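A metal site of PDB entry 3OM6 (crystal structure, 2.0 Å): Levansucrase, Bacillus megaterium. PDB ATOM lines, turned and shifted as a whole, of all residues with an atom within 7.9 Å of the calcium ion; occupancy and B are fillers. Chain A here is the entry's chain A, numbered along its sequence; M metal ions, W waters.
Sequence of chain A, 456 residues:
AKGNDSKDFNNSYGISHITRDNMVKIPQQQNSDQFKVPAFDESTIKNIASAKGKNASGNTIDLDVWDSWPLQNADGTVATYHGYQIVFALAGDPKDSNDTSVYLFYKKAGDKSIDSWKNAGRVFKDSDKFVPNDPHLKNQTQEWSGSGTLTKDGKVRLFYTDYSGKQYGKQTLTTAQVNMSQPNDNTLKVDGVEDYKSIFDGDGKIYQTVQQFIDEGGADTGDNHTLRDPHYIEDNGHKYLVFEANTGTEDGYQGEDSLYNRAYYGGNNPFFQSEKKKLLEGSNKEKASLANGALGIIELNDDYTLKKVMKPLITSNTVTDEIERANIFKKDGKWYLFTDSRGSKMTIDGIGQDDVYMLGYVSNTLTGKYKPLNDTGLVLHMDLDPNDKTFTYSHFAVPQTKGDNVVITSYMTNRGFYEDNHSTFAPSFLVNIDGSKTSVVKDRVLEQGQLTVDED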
ATOM      1  N   GLN A 208       5.324 -15.434  15.832  1.00  0.00           N
ATOM      2  CA  GLN A 208       4.885 -14.078  16.190  1.00  0.00           C
ATOM      3  C   GLN A 208       4.417 -13.295  14.964  1.00  0.00           C
ATOM      4  O   GLN A 208       5.066 -13.318  13.925  1.00  0.00           O
ATOM      5  CB  GLN A 208       6.021 -13.328  16.895  1.00  0.00           C
ATOM      6  CG  GLN A 208       5.590 -12.028  17.577  1.00  0.00           C
ATOM      7  CD  GLN A 208       6.765 -11.111  17.897  1.00  0.00           C
ATOM      8  OE1 GLN A 208       7.633 -10.868  17.061  1.00  0.00           O
ATOM      9  NE2 GLN A 208       6.781 -10.591  19.129  1.00  0.00           N
ATOM     10  N   PHE A 213       3.667  -7.753  17.986  1.00  0.00           N
ATOM     11  CA  PHE A 213       4.824  -6.871  18.149  1.00  0.00           C
ATOM     12  C   PHE A 213       4.369  -5.467  18.546  1.00  0.00           C
ATOM     13  O   PHE A 213       4.856  -4.915  19.533  1.00  0.00           O
ATOM     14  CB  PHE A 213       5.658  -6.854  16.859  1.00  0.00           C
ATOM     15  CG  PHE A 213       6.708  -5.774  16.823  1.00  0.00           C
ATOM     16  CD1 PHE A 213       7.926  -5.938  17.484  1.00  0.00           C
ATOM     17  CD2 PHE A 213       6.486  -4.593  16.119  1.00  0.00           C
ATOM     18  CE1 PHE A 213       8.893  -4.932  17.444  1.00  0.00           C
ATOM     19  CE2 PHE A 213       7.447  -3.592  16.063  1.00  0.00           C
ATOM     20  CZ  PHE A 213       8.655  -3.763  16.737  1.00  0.00           C
ATOM     21  N   GLY A 222      12.330  -2.140  22.316  1.00  0.00           N
ATOM     22  CA  GLY A 222      13.507  -2.623  21.615  1.00  0.00           C
ATOM     23  C   GLY A 222      13.345  -4.056  21.150  1.00  0.00           C
ATOM     24  O   GLY A 222      14.323  -4.795  21.012  1.00  0.00           O
ATOM     25  N   ASP A 223      12.101  -4.446  20.903  1.00  0.00           N
ATOM     26  CA  ASP A 223      11.775  -5.776  20.407  1.00  0.00           C
ATOM     27  C   ASP A 223      12.109  -5.868  18.919  1.00  0.00           C
ATOM     28  O   ASP A 223      12.058  -4.861  18.202  1.00  0.00           O
ATOM     29  CB  ASP A 223      10.294  -6.093  20.647  1.00  0.00           C
ATOM     30  CG  ASP A 223       9.993  -7.582  20.618  1.00  0.00           C
ATOM     31  OD1 ASP A 223      10.870  -8.395  20.981  1.00  0.00           O
ATOM     32  OD2 ASP A 223       8.863  -7.949  20.222  1.00  0.00           O
ATOM     33  N   ASN A 224      12.469  -7.061  18.462  1.00  0.00           N
ATOM     34  CA  ASN A 224      12.785  -7.279  17.064  1.00  0.00           C
ATOM     35  C   ASN A 224      11.877  -8.329  16.432  1.00  0.00           C
ATOM     36  O   ASN A 224      12.021  -9.525  16.672  1.00  0.00           O
ATOM     37  CB  ASN A 224      14.270  -7.658  16.910  1.00  0.00           C
ATOM     38  CG  ASN A 224      14.677  -7.923  15.468  1.00  0.00           C
ATOM     39  OD1 ASN A 224      14.064  -7.428  14.528  1.00  0.00           O
ATOM     40  ND2 ASN A 224      15.721  -8.711  15.296  1.00  0.00           N
ATOM     41  N   HIS A 225      10.940  -7.864  15.612  1.00  0.00           N
ATOM     42  CA  HIS A 225      10.039  -8.752  14.885  1.00  0.00           C
ATOM     43  C   HIS A 225      10.649  -9.189  13.565  1.00  0.00           C
ATOM     44  O   HIS A 225      11.064  -8.348  12.753  1.00  0.00           O
ATOM     45  CB  HIS A 225       8.681  -8.085  14.659  1.00  0.00           C
ATOM     46  CG  HIS A 225       7.761  -8.879  13.768  1.00  0.00           C
ATOM     47  ND1 HIS A 225       7.079  -9.990  14.206  1.00  0.00           N
ATOM     48  CD2 HIS A 225       7.426  -8.716  12.467  1.00  0.00           C
ATOM     49  CE1 HIS A 225       6.367 -10.483  13.219  1.00  0.00           C
ATOM     50  NE2 HIS A 225       6.554  -9.732  12.145  1.00  0.00           N
ATOM     51  N   THR A 226      10.700 -10.507  13.348  1.00  0.00           N
ATOM     52  CA  THR A 226      11.264 -11.066  12.122  1.00  0.00           C
ATOM     53  C   THR A 226      10.368 -12.170  11.551  1.00  0.00           C
ATOM     54  O   THR A 226       9.838 -13.002  12.292  1.00  0.00           O
ATOM     55  CB  THR A 226      12.675 -11.669  12.356  1.00  0.00           C
ATOM     56  OG1 THR A 226      12.587 -12.819  13.203  1.00  0.00           O
ATOM     57  CG2 THR A 226      13.625 -10.641  12.976  1.00  0.00           C
ATOM     58  N   ALA A 245      12.252 -16.481  12.166  1.00  0.00           N
ATOM     59  CA  ALA A 245      11.011 -16.048  12.803  1.00  0.00           C
ATOM     60  C   ALA A 245      11.186 -15.786  14.298  1.00  0.00           C
ATOM     61  O   ALA A 245      12.301 -15.793  14.820  1.00  0.00           O
ATOM     62  CB  ALA A 245       9.894 -17.072  12.557  1.00  0.00           C
ATOM     63  N   ASN A 246      10.065 -15.520  14.966  1.00  0.00           N
ATOM     64  CA  ASN A 246      10.026 -15.379  16.413  1.00  0.00           C
ATOM     65  C   ASN A 246       8.887 -16.232  16.958  1.00  0.00           C
ATOM     66  O   ASN A 246       7.873 -16.401  16.292  1.00  0.00           O
ATOM     67  CB  ASN A 246       9.849 -13.912  16.802  1.00  0.00           C
ATOM     68  CG  ASN A 246      11.038 -13.053  16.414  1.00  0.00           C
ATOM     69  OD1 ASN A 246      11.029 -12.388  15.378  1.00  0.00           O
ATOM     70  ND2 ASN A 246      12.086 -13.089  17.234  1.00  0.00           N
ATOM     71  N   THR A 247       9.078 -16.768  18.169  1.00  0.00           N
ATOM     72  CA  THR A 247       8.091 -17.689  18.741  1.00  0.00           C
ATOM     73  C   THR A 247       6.747 -17.008  18.991  1.00  0.00           C
ATOM     74  O   THR A 247       6.679 -15.798  19.229  1.00  0.00           O
ATOM     75  CB  THR A 247       8.586 -18.327  20.066  1.00  0.00           C
ATOM     76  OG1 THR A 247       8.768 -17.316  21.066  1.00  0.00           O
ATOM     77  CG2 THR A 247       9.903 -19.071  19.855  1.00  0.00           C
ATOM     78  N   TYR A 253       6.900 -18.239  24.416  1.00  0.00           N
ATOM     79  CA  TYR A 253       6.801 -16.812  24.086  1.00  0.00           C
ATOM     80  C   TYR A 253       7.837 -15.968  24.839  1.00  0.00           C
ATOM     81  O   TYR A 253       8.357 -16.392  25.876  1.00  0.00           O
ATOM     82  CB  TYR A 253       5.386 -16.310  24.385  1.00  0.00           C
ATOM     83  CG  TYR A 253       4.983 -15.015  23.700  1.00  0.00           C
ATOM     84  CD1 TYR A 253       5.163 -14.846  22.329  1.00  0.00           C
ATOM     85  CD2 TYR A 253       4.394 -13.979  24.418  1.00  0.00           C
ATOM     86  CE1 TYR A 253       4.793 -13.666  21.692  1.00  0.00           C
ATOM     87  CE2 TYR A 253       4.014 -12.789  23.795  1.00  0.00           C
ATOM     88  CZ  TYR A 253       4.213 -12.650  22.430  1.00  0.00           C
ATOM     89  OH  TYR A 253       3.833 -11.478  21.806  1.00  0.00           O
ATOM     90  N   GLN A 254       8.118 -14.796  24.292  1.00  0.00           N
ATOM     91  CA  GLN A 254       8.982 -13.811  24.939  1.00  0.00           C
ATOM     92  C   GLN A 254       8.337 -13.276  26.224  1.00  0.00           C
ATOM     93  O   GLN A 254       7.128 -13.404  26.420  1.00  0.00           O
ATOM     94  CB  GLN A 254       9.282 -12.650  23.977  1.00  0.00           C
ATOM     95  CG  GLN A 254       8.048 -11.892  23.504  1.00  0.00           C
ATOM     96  CD  GLN A 254       8.332 -10.926  22.374  1.00  0.00           C
ATOM     97  OE1 GLN A 254       8.997 -11.275  21.393  1.00  0.00           O
ATOM     98  NE2 GLN A 254       7.834  -9.700  22.501  1.00  0.00           N
ATOM     99  N   GLY A 255       9.163 -12.675  27.073  1.00  0.00           N
ATOM    100  CA  GLY A 255       8.703 -12.159  28.358  1.00  0.00           C
ATOM    101  C   GLY A 255       9.599 -12.592  29.506  1.00  0.00           C
ATOM    102  O   GLY A 255      10.591 -13.293  29.295  1.00  0.00           O
ATOM    103  N   GLU A 286      15.621  -6.867  30.053  1.00  0.00           N
ATOM    104  CA  GLU A 286      14.625  -6.660  29.009  1.00  0.00           C
ATOM    105  C   GLU A 286      15.057  -7.307  27.698  1.00  0.00           C
ATOM    106  O   GLU A 286      14.251  -7.977  27.038  1.00  0.00           O
ATOM    107  CB  GLU A 286      14.354  -5.165  28.808  1.00  0.00           C
ATOM    108  CG  GLU A 286      13.215  -4.862  27.836  1.00  0.00           C
ATOM    109  CD  GLU A 286      12.862  -3.393  27.765  1.00  0.00           C
ATOM    110  OE1 GLU A 286      13.748  -2.573  27.421  1.00  0.00           O
ATOM    111  OE2 GLU A 286      11.697  -3.053  28.043  1.00  0.00           O
ATOM    112  N   LYS A 287      16.322  -7.103  27.332  1.00  0.00           N
ATOM    113  CA  LYS A 287      16.890  -7.649  26.101  1.00  0.00           C
ATOM    114  C   LYS A 287      16.753  -9.170  26.038  1.00  0.00           C
ATOM    115  O   LYS A 287      16.302  -9.714  25.028  1.00  0.00           O
ATOM    116  CB  LYS A 287      18.359  -7.240  25.970  1.00  0.00           C
ATOM    117  CG  LYS A 287      18.980  -7.481  24.601  1.00  0.00           C
ATOM    118  CD  LYS A 287      20.385  -6.928  24.536  1.00  0.00           C
ATOM    119  CE  LYS A 287      20.997  -7.097  23.153  1.00  0.00           C
ATOM    120  NZ  LYS A 287      22.303  -6.406  23.049  1.00  0.00           N
ATOM    121  N   ALA A 288      17.143  -9.849  27.122  1.00  0.00           N
ATOM    122  CA  ALA A 288      17.013 -11.300  27.211  1.00  0.00           C
ATOM    123  C   ALA A 288      15.553 -11.760  27.230  1.00  0.00           C
ATOM    124  O   ALA A 288      15.216 -12.768  26.612  1.00  0.00           O
ATOM    125  CB  ALA A 288      17.756 -11.824  28.445  1.00  0.00           C
ATOM    126  N   SER A 289      14.695 -11.004  27.917  1.00  0.00           N
ATOM    127  CA  SER A 289      13.267 -11.314  27.992  1.00  0.00           C
ATOM    128  C   SER A 289      12.581 -11.229  26.630  1.00  0.00           C
ATOM    129  O   SER A 289      11.750 -12.070  26.298  1.00  0.00           O
ATOM    130  CB  SER A 289      12.563 -10.391  28.991  1.00  0.00           C
ATOM    131  OG  SER A 289      12.999 -10.640  30.324  1.00  0.00           O
ATOM    132  N   LEU A 290      12.957 -10.217  25.854  1.00  0.00           N
ATOM    133  CA  LEU A 290      12.393 -10.014  24.521  1.00  0.00           C
ATOM    134  C   LEU A 290      12.992 -10.948  23.472  1.00  0.00           C
ATOM    135  O   LEU A 290      12.398 -11.159  22.410  1.00  0.00           O
ATOM    136  CB  LEU A 290      12.551  -8.551  24.077  1.00  0.00           C
ATOM    137  CG  LEU A 290      11.629  -7.512  24.731  1.00  0.00           C
ATOM    138  CD1 LEU A 290      12.097  -6.105  24.400  1.00  0.00           C
ATOM    139  CD2 LEU A 290      10.178  -7.713  24.321  1.00  0.00           C
ATOM    140  N   ALA A 291      14.170 -11.500  23.775  1.00  0.00           N
ATOM    141  CA  ALA A 291      14.864 -12.415  22.862  1.00  0.00           C
ATOM    142  C   ALA A 291      14.118 -13.735  22.701  1.00  0.00           C
ATOM    143  O   ALA A 291      14.132 -14.583  23.603  1.00  0.00           O
ATOM    144  CB  ALA A 291      16.288 -12.647  23.348  1.00  0.00           C
ATOM    145  N   ASN A 292      13.469 -13.913  21.550  1.00  0.00           N
ATOM    146  CA  ASN A 292      12.767 -15.165  21.244  1.00  0.00           C
ATOM    147  C   ASN A 292      12.867 -15.582  19.767  1.00  0.00           C
ATOM    148  O   ASN A 292      11.882 -15.990  19.163  1.00  0.00           O
ATOM    149  CB  ASN A 292      11.304 -15.115  21.730  1.00  0.00           C
ATOM    150  CG  ASN A 292      10.438 -14.162  20.910  1.00  0.00           C
ATOM    151  OD1 ASN A 292      10.924 -13.241  20.260  1.00  0.00           O
ATOM    152  ND2 ASN A 292       9.125 -14.391  20.938  1.00  0.00           N
ATOM    153  N   GLY A 293      14.074 -15.489  19.215  1.00  0.00           N
ATOM    154  CA  GLY A 293      14.330 -15.913  17.836  1.00  0.00           C
ATOM    155  C   GLY A 293      14.016 -17.371  17.593  1.00  0.00           C
ATOM    156  O   GLY A 293      14.111 -18.198  18.507  1.00  0.00           O
ATOM    157  N   THR A 320      19.177 -14.573  21.840  1.00  0.00           N
ATOM    158  CA  THR A 320      19.057 -13.479  20.874  1.00  0.00           C
ATOM    159  C   THR A 320      17.669 -13.451  20.233  1.00  0.00           C
ATOM    160  O   THR A 320      16.954 -14.460  20.197  1.00  0.00           O
ATOM    161  CB  THR A 320      20.169 -13.516  19.785  1.00  0.00           C
ATOM    162  OG1 THR A 320      19.959 -12.459  18.839  1.00  0.00           O
ATOM    163  CG2 THR A 320      20.190 -14.850  19.054  1.00  0.00           C
ATOM    164  N   ASP A 321      17.289 -12.282  19.737  1.00  0.00           N
ATOM    165  CA  ASP A 321      16.006 -12.094  19.070  1.00  0.00           C
ATOM    166  C   ASP A 321      16.175 -12.187  17.553  1.00  0.00           C
ATOM    167  O   ASP A 321      15.190 -12.084  16.800  1.00  0.00           O
ATOM    168  CB  ASP A 321      15.401 -10.734  19.450  1.00  0.00           C
ATOM    169  CG  ASP A 321      13.892 -10.737  19.435  1.00  0.00           C
ATOM    170  OD1 ASP A 321      13.295 -11.835  19.362  1.00  0.00           O
ATOM    171  OD2 ASP A 321      13.289  -9.651  19.519  1.00  0.00           O
ATOM    172  N   GLU A 322      17.412 -12.387  17.115  1.00  0.00           N
ATOM    173  CA  GLU A 322      17.736 -12.358  15.689  1.00  0.00           C
ATOM    174  C   GLU A 322      18.701 -13.477  15.275  1.00  0.00           C
ATOM    175  O   GLU A 322      19.909 -13.386  15.498  1.00  0.00           O
ATOM    176  CB  GLU A 322      18.304 -10.992  15.315  1.00  0.00           C
ATOM    177  CG  GLU A 322      18.179 -10.653  13.839  1.00  0.00           C
ATOM    178  CD  GLU A 322      18.667  -9.258  13.516  1.00  0.00           C
ATOM    179  OE1 GLU A 322      17.904  -8.471  12.927  1.00  0.00           O
ATOM    180  OE2 GLU A 322      19.835  -8.950  13.866  1.00  0.00           O
HETATM  181 CA    CA M   1      11.145 -10.830  20.414  1.00  0.00          CA
HETATM  182  O   HOH W   1      10.150 -10.628  18.251  1.00  0.00           O
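Five residues have an atom within 4 Å of the calcium ion: Asp 223, Gln 254, Leu 290, Asn 292 and Asp 321.
Water W1 lies within hydrogen-bond range of the backbone carbonyl oxygen of Asn 224 (2.7 Å), the side-chain amide oxygen of Gln 208 (2.8 Å) and the side-chain amide nitrogen of Asn 246 (3.3 Å).
The side-chain amide oxygen (OE1) of Gln 254 lies close to the side-chain amide nitrogen (NE2) of Gln 208, at 3.2 Å. ND2 of Asn 246 sits close to O of Asn 292, at 3.5 Å. ND2 of Asn 292 sits at hydrogen-bond distance from OG1 of Thr 247 (2.9 Å). The backbone carbonyl oxygen (O) of Asp 321 is in hydrogen-bond range of the side-chain amide nitrogen (ND2) of Asn 246 (3.3 Å). The side-chain carboxylate (OD2) of Asp 321 sits close to the backbone NH (N) of Asn 224, 2.9 Å away.
The calcium ion is bound by O of Leu 290, water W1, OE1 of Gln 254, OD1 of Asn 292, OD1 of Asp 223, OD1 of Asp 321 and OD2 of Asp 321.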
